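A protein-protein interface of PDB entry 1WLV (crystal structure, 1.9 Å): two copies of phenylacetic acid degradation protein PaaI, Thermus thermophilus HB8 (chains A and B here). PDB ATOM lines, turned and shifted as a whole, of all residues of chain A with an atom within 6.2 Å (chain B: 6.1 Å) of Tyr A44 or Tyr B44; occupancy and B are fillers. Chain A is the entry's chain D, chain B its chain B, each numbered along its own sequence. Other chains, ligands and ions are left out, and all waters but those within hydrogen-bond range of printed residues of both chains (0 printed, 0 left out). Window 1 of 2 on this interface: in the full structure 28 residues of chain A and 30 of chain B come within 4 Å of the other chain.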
ATOM      1  N   HIS A  39      12.251 -16.210 -30.037  1.00  0.00           N
ATOM      2  CA  HIS A  39      12.084 -15.257 -28.945  1.00  0.00           C
ATOM      3  C   HIS A  39      11.166 -14.122 -29.408  1.00  0.00           C
ATOM      4  O   HIS A  39      11.269 -13.654 -30.542  1.00  0.00           O
ATOM      5  CB  HIS A  39      13.454 -14.708 -28.536  1.00  0.00           C
ATOM      6  CG  HIS A  39      13.465 -13.998 -27.219  1.00  0.00           C
ATOM      7  ND1 HIS A  39      12.840 -12.784 -27.018  1.00  0.00           N
ATOM      8  CD2 HIS A  39      14.058 -14.314 -26.043  1.00  0.00           C
ATOM      9  CE1 HIS A  39      13.053 -12.382 -25.779  1.00  0.00           C
ATOM     10  NE2 HIS A  39      13.790 -13.291 -25.166  1.00  0.00           N
ATOM     11  N   GLY A  40      10.256 -13.695 -28.536  1.00  0.00           N
ATOM     12  CA  GLY A  40       9.343 -12.621 -28.891  1.00  0.00           C
ATOM     13  C   GLY A  40      10.084 -11.352 -29.268  1.00  0.00           C
ATOM     14  O   GLY A  40       9.593 -10.545 -30.062  1.00  0.00           O
ATOM     15  N   GLY A  41      11.267 -11.175 -28.686  1.00  0.00           N
ATOM     16  CA  GLY A  41      12.079 -10.004 -28.969  1.00  0.00           C
ATOM     17  C   GLY A  41      12.695 -10.065 -30.355  1.00  0.00           C
ATOM     18  O   GLY A  41      12.951  -9.034 -30.964  1.00  0.00           O
ATOM     19  N   PHE A  42      12.956 -11.267 -30.855  1.00  0.00           N
ATOM     20  CA  PHE A  42      13.529 -11.399 -32.196  1.00  0.00           C
ATOM     21  C   PHE A  42      12.451 -11.057 -33.226  1.00  0.00           C
ATOM     22  O   PHE A  42      12.691 -10.304 -34.168  1.00  0.00           O
ATOM     23  CB  PHE A  42      14.038 -12.826 -32.441  1.00  0.00           C
ATOM     24  CG  PHE A  42      14.529 -13.055 -33.845  1.00  0.00           C
ATOM     25  CD1 PHE A  42      15.710 -12.459 -34.289  1.00  0.00           C
ATOM     26  CD2 PHE A  42      13.786 -13.819 -34.740  1.00  0.00           C
ATOM     27  CE1 PHE A  42      16.142 -12.618 -35.601  1.00  0.00           C
ATOM     28  CE2 PHE A  42      14.211 -13.985 -36.066  1.00  0.00           C
ATOM     29  CZ  PHE A  42      15.391 -13.382 -36.493  1.00  0.00           C
ATOM     30  N   LEU A  43      11.257 -11.613 -33.046  1.00  0.00           N
ATOM     31  CA  LEU A  43      10.158 -11.335 -33.966  1.00  0.00           C
ATOM     32  C   LEU A  43       9.822  -9.848 -33.934  1.00  0.00           C
ATOM     33  O   LEU A  43       9.485  -9.258 -34.961  1.00  0.00           O
ATOM     34  CB  LEU A  43       8.915 -12.147 -33.586  1.00  0.00           C
ATOM     35  CG  LEU A  43       9.062 -13.669 -33.670  1.00  0.00           C
ATOM     36  CD1 LEU A  43       7.749 -14.331 -33.296  1.00  0.00           C
ATOM     37  CD2 LEU A  43       9.474 -14.073 -35.075  1.00  0.00           C
ATOM     38  N   TYR A  44       9.906  -9.244 -32.752  1.00  0.00           N
ATOM     39  CA  TYR A  44       9.615  -7.821 -32.633  1.00  0.00           C
ATOM     40  C   TYR A  44      10.702  -7.010 -33.324  1.00  0.00           C
ATOM     41  O   TYR A  44      10.410  -6.054 -34.044  1.00  0.00           O
ATOM     42  CB  TYR A  44       9.510  -7.400 -31.162  1.00  0.00           C
ATOM     43  CG  TYR A  44       9.295  -5.906 -30.982  1.00  0.00           C
ATOM     44  CD1 TYR A  44      10.369  -5.014 -30.989  1.00  0.00           C
ATOM     45  CD2 TYR A  44       8.009  -5.383 -30.828  1.00  0.00           C
ATOM     46  CE1 TYR A  44      10.167  -3.628 -30.843  1.00  0.00           C
ATOM     47  CE2 TYR A  44       7.798  -4.003 -30.681  1.00  0.00           C
ATOM     48  CZ  TYR A  44       8.878  -3.135 -30.688  1.00  0.00           C
ATOM     49  OH  TYR A  44       8.664  -1.776 -30.522  1.00  0.00           O
ATOM     50  N   ALA A  45      11.957  -7.389 -33.105  1.00  0.00           N
ATOM     51  CA  ALA A  45      13.076  -6.676 -33.718  1.00  0.00           C
ATOM     52  C   ALA A  45      12.932  -6.661 -35.242  1.00  0.00           C
ATOM     53  O   ALA A  45      13.277  -5.678 -35.904  1.00  0.00           O
ATOM     54  CB  ALA A  45      14.394  -7.334 -33.319  1.00  0.00           C
ATOM     55  N   LEU A  46      12.424  -7.760 -35.790  1.00  0.00           N
ATOM     56  CA  LEU A  46      12.220  -7.878 -37.230  1.00  0.00           C
ATOM     57  C   LEU A  46      11.133  -6.909 -37.696  1.00  0.00           C
ATOM     58  O   LEU A  46      11.318  -6.158 -38.659  1.00  0.00           O
ATOM     59  CB  LEU A  46      11.820  -9.314 -37.578  1.00  0.00           C
ATOM     60  CG  LEU A  46      11.399  -9.608 -39.021  1.00  0.00           C
ATOM     61  CD1 LEU A  46      12.552  -9.355 -39.972  1.00  0.00           C
ATOM     62  CD2 LEU A  46      10.940 -11.047 -39.117  1.00  0.00           C
ATOM     63  N   ALA A  47       9.998  -6.928 -37.009  1.00  0.00           N
ATOM     64  CA  ALA A  47       8.894  -6.043 -37.360  1.00  0.00           C
ATOM     65  C   ALA A  47       9.290  -4.585 -37.146  1.00  0.00           C
ATOM     66  O   ALA A  47       8.989  -3.719 -37.975  1.00  0.00           O
ATOM     67  CB  ALA A  47       7.657  -6.388 -36.517  1.00  0.00           C
ATOM     68  N   ASP A  48       9.969  -4.318 -36.034  1.00  0.00           N
ATOM     69  CA  ASP A  48      10.399  -2.964 -35.701  1.00  0.00           C
ATOM     70  C   ASP A  48      11.371  -2.411 -36.742  1.00  0.00           C
ATOM     71  O   ASP A  48      11.390  -1.206 -37.006  1.00  0.00           O
ATOM     72  CB  ASP A  48      11.062  -2.944 -34.318  1.00  0.00           C
ATOM     73  CG  ASP A  48      11.396  -1.540 -33.855  1.00  0.00           C
ATOM     74  OD1 ASP A  48      10.456  -0.730 -33.702  1.00  0.00           O
ATOM     75  OD2 ASP A  48      12.592  -1.244 -33.644  1.00  0.00           O
ATOM     76  N   SER A  49      12.181  -3.291 -37.323  1.00  0.00           N
ATOM     77  CA  SER A  49      13.138  -2.879 -38.347  1.00  0.00           C
ATOM     78  C   SER A  49      12.422  -2.473 -39.640  1.00  0.00           C
ATOM     79  O   SER A  49      12.787  -1.479 -40.270  1.00  0.00           O
ATOM     80  CB  SER A  49      14.134  -4.005 -38.632  1.00  0.00           C
ATOM     81  OG  SER A  49      14.962  -4.241 -37.509  1.00  0.00           O
ATOM     82  N   PHE A  51       9.409  -1.474 -39.760  1.00  0.00           N
ATOM     83  CA  PHE A  51       8.704  -0.278 -39.301  1.00  0.00           C
ATOM     84  C   PHE A  51       9.630   0.937 -39.411  1.00  0.00           C
ATOM     85  O   PHE A  51       9.253   1.964 -39.975  1.00  0.00           O
ATOM     86  CB  PHE A  51       8.252  -0.511 -37.847  1.00  0.00           C
ATOM     87  CG  PHE A  51       7.878   0.739 -37.089  1.00  0.00           C
ATOM     88  CD1 PHE A  51       6.816   1.544 -37.497  1.00  0.00           C
ATOM     89  CD2 PHE A  51       8.559   1.071 -35.916  1.00  0.00           C
ATOM     90  CE1 PHE A  51       6.435   2.661 -36.746  1.00  0.00           C
ATOM     91  CE2 PHE A  51       8.189   2.179 -35.158  1.00  0.00           C
ATOM     92  CZ  PHE A  51       7.125   2.977 -35.571  1.00  0.00           C
ATOM     93  N   SER A  65       5.083   4.713 -29.914  1.00  0.00           N
ATOM     94  CA  SER A  65       4.410   3.561 -29.320  1.00  0.00           C
ATOM     95  C   SER A  65       4.198   2.437 -30.327  1.00  0.00           C
ATOM     96  O   SER A  65       3.752   2.670 -31.453  1.00  0.00           O
ATOM     97  CB  SER A  65       3.049   3.986 -28.758  1.00  0.00           C
ATOM     98  OG  SER A  65       2.389   2.888 -28.153  1.00  0.00           O
ATOM     99  N   CYS A  66       4.517   1.215 -29.912  1.00  0.00           N
ATOM    100  CA  CYS A  66       4.349   0.050 -30.768  1.00  0.00           C
ATOM    101  C   CYS A  66       3.614  -1.049 -30.007  1.00  0.00           C
ATOM    102  O   CYS A  66       3.760  -1.182 -28.792  1.00  0.00           O
ATOM    103  CB  CYS A  66       5.711  -0.475 -31.224  1.00  0.00           C
ATOM    104  SG  CYS A  66       6.749   0.783 -32.007  1.00  0.00           S
ATOM    105  N   ARG A  67       2.817  -1.822 -30.735  1.00  0.00           N
ATOM    106  CA  ARG A  67       2.077  -2.936 -30.161  1.00  0.00           C
ATOM    107  C   ARG A  67       2.456  -4.173 -30.957  1.00  0.00           C
ATOM    108  O   ARG A  67       2.610  -4.117 -32.178  1.00  0.00           O
ATOM    109  CB  ARG A  67       0.565  -2.711 -30.265  1.00  0.00           C
ATOM    110  CG  ARG A  67      -0.288  -3.909 -29.808  1.00  0.00           C
ATOM    111  CD  ARG A  67      -1.782  -3.635 -30.023  1.00  0.00           C
ATOM    112  NE  ARG A  67      -2.636  -4.793 -29.734  1.00  0.00           N
ATOM    113  CZ  ARG A  67      -3.392  -4.928 -28.650  1.00  0.00           C
ATOM    114  NH1 ARG A  67      -3.416  -3.977 -27.721  1.00  0.00           N
ATOM    115  NH2 ARG A  67      -4.146  -6.012 -28.503  1.00  0.00           N
ATOM    116  N   MET A  68       2.612  -5.287 -30.258  1.00  0.00           N
ATOM    117  CA  MET A  68       2.956  -6.538 -30.904  1.00  0.00           C
ATOM    118  C   MET A  68       1.994  -7.625 -30.436  1.00  0.00           C
ATOM    119  O   MET A  68       1.927  -7.927 -29.246  1.00  0.00           O
ATOM    120  CB  MET A  68       4.388  -6.935 -30.551  1.00  0.00           C
ATOM    121  CG  MET A  68       4.847  -8.217 -31.210  1.00  0.00           C
ATOM    122  SD  MET A  68       5.282  -8.008 -32.943  1.00  0.00           S
ATOM    123  CE  MET A  68       6.359  -9.397 -33.164  1.00  0.00           C
ATOM    124  N   TYR A  70       1.073 -11.560 -30.779  1.00  0.00           N
ATOM    125  CA  TYR A  70       1.621 -12.855 -31.189  1.00  0.00           C
ATOM    126  C   TYR A  70       0.533 -13.899 -31.429  1.00  0.00           C
ATOM    127  O   TYR A  70      -0.311 -14.132 -30.559  1.00  0.00           O
ATOM    128  CB  TYR A  70       2.580 -13.365 -30.113  1.00  0.00           C
ATOM    129  CG  TYR A  70       3.757 -12.452 -29.865  1.00  0.00           C
ATOM    130  CD1 TYR A  70       4.899 -12.526 -30.662  1.00  0.00           C
ATOM    131  CD2 TYR A  70       3.743 -11.532 -28.816  1.00  0.00           C
ATOM    132  CE1 TYR A  70       6.007 -11.711 -30.415  1.00  0.00           C
ATOM    133  CE2 TYR A  70       4.845 -10.709 -28.561  1.00  0.00           C
ATOM    134  CZ  TYR A  70       5.972 -10.807 -29.363  1.00  0.00           C
ATOM    135  OH  TYR A  70       7.068 -10.008 -29.111  1.00  0.00           O
ATOM    136  N   PHE A 110       2.122  -6.263 -35.893  1.00  0.00           N
ATOM    137  CA  PHE A 110       2.779  -5.135 -35.237  1.00  0.00           C
ATOM    138  C   PHE A 110       2.097  -3.848 -35.703  1.00  0.00           C
ATOM    139  O   PHE A 110       1.719  -3.719 -36.866  1.00  0.00           O
ATOM    140  CB  PHE A 110       4.278  -5.167 -35.610  1.00  0.00           C
ATOM    141  CG  PHE A 110       5.070  -3.937 -35.211  1.00  0.00           C
ATOM    142  CD1 PHE A 110       4.915  -2.734 -35.893  1.00  0.00           C
ATOM    143  CD2 PHE A 110       6.027  -4.011 -34.200  1.00  0.00           C
ATOM    144  CE1 PHE A 110       5.704  -1.620 -35.583  1.00  0.00           C
ATOM    145  CE2 PHE A 110       6.825  -2.904 -33.879  1.00  0.00           C
ATOM    146  CZ  PHE A 110       6.664  -1.708 -34.573  1.00  0.00           C
ATOM    147  N   HIS B  39      18.743   0.495 -30.782  1.00  0.00           N
ATOM    148  CA  HIS B  39      17.662   0.071 -31.662  1.00  0.00           C
ATOM    149  C   HIS B  39      16.418  -0.233 -30.821  1.00  0.00           C
ATOM    150  O   HIS B  39      16.521  -0.787 -29.728  1.00  0.00           O
ATOM    151  CB  HIS B  39      18.123  -1.171 -32.431  1.00  0.00           C
ATOM    152  CG  HIS B  39      17.224  -1.570 -33.558  1.00  0.00           C
ATOM    153  ND1 HIS B  39      15.979  -2.128 -33.360  1.00  0.00           N
ATOM    154  CD2 HIS B  39      17.415  -1.546 -34.898  1.00  0.00           C
ATOM    155  CE1 HIS B  39      15.445  -2.435 -34.528  1.00  0.00           C
ATOM    156  NE2 HIS B  39      16.296  -2.093 -35.478  1.00  0.00           N
ATOM    157  N   GLY B  40      15.248   0.144 -31.325  1.00  0.00           N
ATOM    158  CA  GLY B  40      14.019  -0.105 -30.589  1.00  0.00           C
ATOM    159  C   GLY B  40      13.808  -1.579 -30.297  1.00  0.00           C
ATOM    160  O   GLY B  40      13.140  -1.939 -29.326  1.00  0.00           O
ATOM    161  N   GLY B  41      14.376  -2.434 -31.143  1.00  0.00           N
ATOM    162  CA  GLY B  41      14.243  -3.868 -30.958  1.00  0.00           C
ATOM    163  C   GLY B  41      15.057  -4.362 -29.778  1.00  0.00           C
ATOM    164  O   GLY B  41      14.673  -5.329 -29.116  1.00  0.00           O
ATOM    165  N   PHE B  42      16.186  -3.708 -29.519  1.00  0.00           N
ATOM    166  CA  PHE B  42      17.036  -4.090 -28.394  1.00  0.00           C
ATOM    167  C   PHE B  42      16.336  -3.770 -27.074  1.00  0.00           C
ATOM    168  O   PHE B  42      16.263  -4.614 -26.183  1.00  0.00           O
ATOM    169  CB  PHE B  42      18.379  -3.346 -28.435  1.00  0.00           C
ATOM    170  CG  PHE B  42      19.215  -3.552 -27.198  1.00  0.00           C
ATOM    171  CD1 PHE B  42      19.790  -4.792 -26.927  1.00  0.00           C
ATOM    172  CD2 PHE B  42      19.378  -2.524 -26.276  1.00  0.00           C
ATOM    173  CE1 PHE B  42      20.514  -5.003 -25.745  1.00  0.00           C
ATOM    174  CE2 PHE B  42      20.097  -2.725 -25.095  1.00  0.00           C
ATOM    175  CZ  PHE B  42      20.664  -3.965 -24.831  1.00  0.00           C
ATOM    176  N   LEU B  43      15.837  -2.544 -26.942  1.00  0.00           N
ATOM    177  CA  LEU B  43      15.158  -2.146 -25.712  1.00  0.00           C
ATOM    178  C   LEU B  43      13.925  -3.019 -25.485  1.00  0.00           C
ATOM    179  O   LEU B  43      13.629  -3.415 -24.356  1.00  0.00           O
ATOM    180  CB  LEU B  43      14.762  -0.667 -25.773  1.00  0.00           C
ATOM    181  CG  LEU B  43      15.926   0.320 -25.910  1.00  0.00           C
ATOM    182  CD1 LEU B  43      15.378   1.735 -26.003  1.00  0.00           C
ATOM    183  CD2 LEU B  43      16.870   0.179 -24.717  1.00  0.00           C
ATOM    184  N   TYR B  44      13.196  -3.312 -26.556  1.00  0.00           N
ATOM    185  CA  TYR B  44      12.022  -4.159 -26.417  1.00  0.00           C
ATOM    186  C   TYR B  44      12.455  -5.550 -25.972  1.00  0.00           C
ATOM    187  O   TYR B  44      11.849  -6.130 -25.074  1.00  0.00           O
ATOM    188  CB  TYR B  44      11.261  -4.264 -27.737  1.00  0.00           C
ATOM    189  CG  TYR B  44      10.062  -5.187 -27.679  1.00  0.00           C
ATOM    190  CD1 TYR B  44      10.207  -6.571 -27.825  1.00  0.00           C
ATOM    191  CD2 TYR B  44       8.778  -4.674 -27.497  1.00  0.00           C
ATOM    192  CE1 TYR B  44       9.094  -7.419 -27.798  1.00  0.00           C
ATOM    193  CE2 TYR B  44       7.663  -5.510 -27.469  1.00  0.00           C
ATOM    194  CZ  TYR B  44       7.829  -6.877 -27.623  1.00  0.00           C
ATOM    195  OH  TYR B  44       6.724  -7.694 -27.626  1.00  0.00           O
ATOM    196  N   ALA B  45      13.504  -6.084 -26.600  1.00  0.00           N
ATOM    197  CA  ALA B  45      13.991  -7.419 -26.255  1.00  0.00           C
ATOM    198  C   ALA B  45      14.327  -7.500 -24.772  1.00  0.00           C
ATOM    199  O   ALA B  45      14.054  -8.507 -24.117  1.00  0.00           O
ATOM    200  CB  ALA B  45      15.227  -7.778 -27.101  1.00  0.00           C
ATOM    201  N   LEU B  46      14.921  -6.438 -24.243  1.00  0.00           N
ATOM    202  CA  LEU B  46      15.269  -6.399 -22.825  1.00  0.00           C
ATOM    203  C   LEU B  46      13.997  -6.479 -21.989  1.00  0.00           C
ATOM    204  O   LEU B  46      13.878  -7.321 -21.100  1.00  0.00           O
ATOM    205  CB  LEU B  46      16.015  -5.106 -22.498  1.00  0.00           C
ATOM    206  CG  LEU B  46      16.187  -4.730 -21.022  1.00  0.00           C
ATOM    207  CD1 LEU B  46      17.043  -5.766 -20.302  1.00  0.00           C
ATOM    208  CD2 LEU B  46      16.837  -3.364 -20.939  1.00  0.00           C
ATOM    209  N   ALA B  47      13.044  -5.597 -22.274  1.00  0.00           N
ATOM    210  CA  ALA B  47      11.787  -5.589 -21.531  1.00  0.00           C
ATOM    211  C   ALA B  47      11.056  -6.923 -21.669  1.00  0.00           C
ATOM    212  O   ALA B  47      10.569  -7.482 -20.683  1.00  0.00           O
ATOM    213  CB  ALA B  47      10.894  -4.456 -22.020  1.00  0.00           C
ATOM    214  N   ASP B  48      10.988  -7.422 -22.898  1.00  0.00           N
ATOM    215  CA  ASP B  48      10.303  -8.675 -23.189  1.00  0.00           C
ATOM    216  C   ASP B  48      10.923  -9.842 -22.429  1.00  0.00           C
ATOM    217  O   ASP B  48      10.220 -10.761 -22.008  1.00  0.00           O
ATOM    218  CB  ASP B  48      10.332  -8.937 -24.701  1.00  0.00           C
ATOM    219  CG  ASP B  48       9.504 -10.143 -25.105  1.00  0.00           C
ATOM    220  OD1 ASP B  48       8.294 -10.177 -24.797  1.00  0.00           O
ATOM    221  OD2 ASP B  48      10.067 -11.059 -25.736  1.00  0.00           O
ATOM    222  N   SER B  49      12.238  -9.801 -22.251  1.00  0.00           N
ATOM    223  CA  SER B  49      12.940 -10.859 -21.529  1.00  0.00           C
ATOM    224  C   SER B  49      12.555 -10.896 -20.048  1.00  0.00           C
ATOM    225  O   SER B  49      12.331 -11.969 -19.483  1.00  0.00           O
ATOM    226  CB  SER B  49      14.453 -10.678 -21.669  1.00  0.00           C
ATOM    227  OG  SER B  49      14.863 -10.923 -23.004  1.00  0.00           O
ATOM    228  N   CYS B  66       1.760  -7.117 -26.420  1.00  0.00           N
ATOM    229  CA  CYS B  66       2.684  -6.265 -25.692  1.00  0.00           C
ATOM    230  C   CYS B  66       2.725  -4.879 -26.316  1.00  0.00           C
ATOM    231  O   CYS B  66       2.577  -4.733 -27.528  1.00  0.00           O
ATOM    232  CB  CYS B  66       4.089  -6.866 -25.715  1.00  0.00           C
ATOM    233  SG  CYS B  66       4.149  -8.572 -25.149  1.00  0.00           S
ATOM    234  N   ARG B  67       2.912  -3.869 -25.474  1.00  0.00           N
ATOM    235  CA  ARG B  67       3.005  -2.485 -25.919  1.00  0.00           C
ATOM    236  C   ARG B  67       4.329  -1.928 -25.418  1.00  0.00           C
ATOM    237  O   ARG B  67       4.759  -2.221 -24.300  1.00  0.00           O
ATOM    238  CB  ARG B  67       1.857  -1.642 -25.356  1.00  0.00           C
ATOM    239  CG  ARG B  67       1.967  -0.142 -25.668  1.00  0.00           C
ATOM    240  CD  ARG B  67       0.836   0.634 -24.990  1.00  0.00           C
ATOM    241  NE  ARG B  67       0.959   2.086 -25.135  1.00  0.00           N
ATOM    242  CZ  ARG B  67       0.240   2.834 -25.967  1.00  0.00           C
ATOM    243  NH1 ARG B  67      -0.673   2.281 -26.756  1.00  0.00           N
ATOM    244  NH2 ARG B  67       0.426   4.150 -25.995  1.00  0.00           N
ATOM    245  N   MET B  68       4.962  -1.117 -26.252  1.00  0.00           N
ATOM    246  CA  MET B  68       6.237  -0.514 -25.912  1.00  0.00           C
ATOM    247  C   MET B  68       6.169   0.978 -26.200  1.00  0.00           C
ATOM    248  O   MET B  68       5.928   1.385 -27.332  1.00  0.00           O
ATOM    249  CB  MET B  68       7.346  -1.156 -26.750  1.00  0.00           C
ATOM    250  CG  MET B  68       8.730  -0.602 -26.483  1.00  0.00           C
ATOM    251  SD  MET B  68       9.392  -1.117 -24.892  1.00  0.00           S
ATOM    252  CE  MET B  68      11.117  -0.795 -25.155  1.00  0.00           C
ATOM    253  N   TYR B  70       8.343   4.410 -26.050  1.00  0.00           N
ATOM    254  CA  TYR B  70       9.722   4.914 -25.989  1.00  0.00           C
ATOM    255  C   TYR B  70       9.778   6.373 -25.538  1.00  0.00           C
ATOM    256  O   TYR B  70       9.086   7.219 -26.102  1.00  0.00           O
ATOM    257  CB  TYR B  70      10.369   4.797 -27.372  1.00  0.00           C
ATOM    258  CG  TYR B  70      10.476   3.381 -27.894  1.00  0.00           C
ATOM    259  CD1 TYR B  70      11.524   2.546 -27.494  1.00  0.00           C
ATOM    260  CD2 TYR B  70       9.534   2.873 -28.788  1.00  0.00           C
ATOM    261  CE1 TYR B  70      11.628   1.240 -27.976  1.00  0.00           C
ATOM    262  CE2 TYR B  70       9.629   1.567 -29.275  1.00  0.00           C
ATOM    263  CZ  TYR B  70      10.678   0.761 -28.867  1.00  0.00           C
ATOM    264  OH  TYR B  70      10.784  -0.524 -29.349  1.00  0.00           O
ATOM    265  N   PHE B 110       6.974  -0.761 -20.872  1.00  0.00           N
ATOM    266  CA  PHE B 110       6.473  -1.945 -21.562  1.00  0.00           C
ATOM    267  C   PHE B 110       5.303  -2.534 -20.770  1.00  0.00           C
ATOM    268  O   PHE B 110       5.342  -2.594 -19.541  1.00  0.00           O
ATOM    269  CB  PHE B 110       7.634  -2.952 -21.691  1.00  0.00           C
ATOM    270  CG  PHE B 110       7.236  -4.321 -22.178  1.00  0.00           C
ATOM    271  CD1 PHE B 110       6.521  -5.194 -21.358  1.00  0.00           C
ATOM    272  CD2 PHE B 110       7.640  -4.765 -23.438  1.00  0.00           C
ATOM    273  CE1 PHE B 110       6.218  -6.496 -21.780  1.00  0.00           C
ATOM    274  CE2 PHE B 110       7.345  -6.063 -23.871  1.00  0.00           C
ATOM    275  CZ  PHE B 110       6.633  -6.930 -23.038  1.00  0.00           C
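Of chain B, only Gly B40 (3.7 Å), Tyr B44 (3.3 Å) and Tyr B70 (2.7 Å) come within 4 Å of Tyr A44.
Of the printed residues of chain B, Ser A49 touches His B39 (3.2 Å).
Of the printed residues of chain B, Met A68 touches Tyr B44 and Cys B66.
Printed residues of chain A within 4 Å of Gly B40: Tyr A44 and Asp A48.
Of chain A, only Gly A40 (3.9 Å), Tyr A44 (3.3 Å), Met A68 (3.8 Å) and Tyr A70 (2.8 Å) come within 4 Å of Tyr B44.
The nearest printed residue of chain A that does not touch Tyr B70 is Cys A66 (4.05 Å).
His A39 touches Asp B48, and with the chains exchanged Asp A48 touches His B39.
Gly A41 touches Asp B48, and with the chains exchanged Asp A48 touches Gly B41.
Tyr A44 touches Tyr B70, and with the chains exchanged Tyr A70 touches Tyr B44.
Met A68 touches Tyr B44, but with the chains exchanged Tyr A44 does not touch Met B68 (4.04 Å).
Positions printed for both chains: 39, 40, 41, 42, 43, 44, 45, 46, 47, 48, 49, 66, 67, 68, 70 and 110.
Of the 21 pairs that touch across the chains among the printed residues, 18 have their exchanged pair printed and touching as well.
Of the 16 printed residues of chain B, 10 touch a printed residue of chain A.
Of the 18 printed residues of chain A, 11 touch a printed residue of chain B.
Among the printed residues, no Asp or Glu carboxylate lies within 4 Å of a Lys or Arg side-chain nitrogen of the other chain.
Among the printed residues, pairs that only touch across the chains: Asp A48 with His B39 (3.2 Å), Arg A67 with Cys B66 (3.2 Å), Cys A66 with Arg B67 (3.2 Å), His A39 with Asp B48 (3.3 Å), Ser A65 with Met B68 (3.3 Å), Tyr A44 with Tyr B44 (3.3 Å), Gly A40 with Asp B48 (3.5 Å), Asp A48 with Gly B40 (3.6 Å), Tyr A44 with Gly B40 (3.7 Å), Met A68 with Tyr B44 (3.8 Å), Gly A40 with Tyr B44 (3.9 Å) and Cys A66 with Cys B66 (3.95 Å).
O of Gly B40 is in hydrogen-bond range of OH of Tyr B70 (2.7 Å).
The side-chain hydroxyl of Tyr B44 sits close to the side-chain sulfur of Cys B66, 3.7 Å away.
The side-chain hydroxyl of Ser B49 is in hydrogen-bond range of the backbone carbonyl oxygen of Ala B45.
A ring nitrogen (ND1) of His A39 is in hydrogen-bond range of the backbone NH of Gly A41 (2.8 Å).
OH of Tyr A70 lies within hydrogen-bond range of O of Gly A40 (2.8 Å).
OH of Tyr A44 lies close to SG of Cys A66 (3.5 Å).
A ring nitrogen (NE2) of His B39 is in hydrogen-bond range of the side-chain hydroxyl (OG) of Ser A49.
N of Gly B41 sits at hydrogen-bond distance from OD2 of Asp A48, 3.3 Å away.
The side-chain hydroxyl (OH) of Tyr A70 sits at hydrogen-bond distance from the side-chain hydroxyl (OH) of Tyr B44 (2.8 Å).
OD2 of Asp B48 sits at hydrogen-bond distance from N of Gly A41 (3.2 Å).
OG of Ser B49 is in hydrogen-bond range of NE2 of His A39 (3.4 Å).
O of Cys B66 is in hydrogen-bond range of N of Met A68, 2.8 Å away.
NH2 of Arg B67 lies close to OG of Ser A65 (3.2 Å).
The backbone carbonyl oxygen (O) of Cys A66 sits at hydrogen-bond distance from the backbone NH (N) of Met B68 (2.8 Å).
The side-chain hydroxyl (OH) of Tyr B70 sits at hydrogen-bond distance from the side-chain hydroxyl (OH) of Tyr A44, at 2.7 Å.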
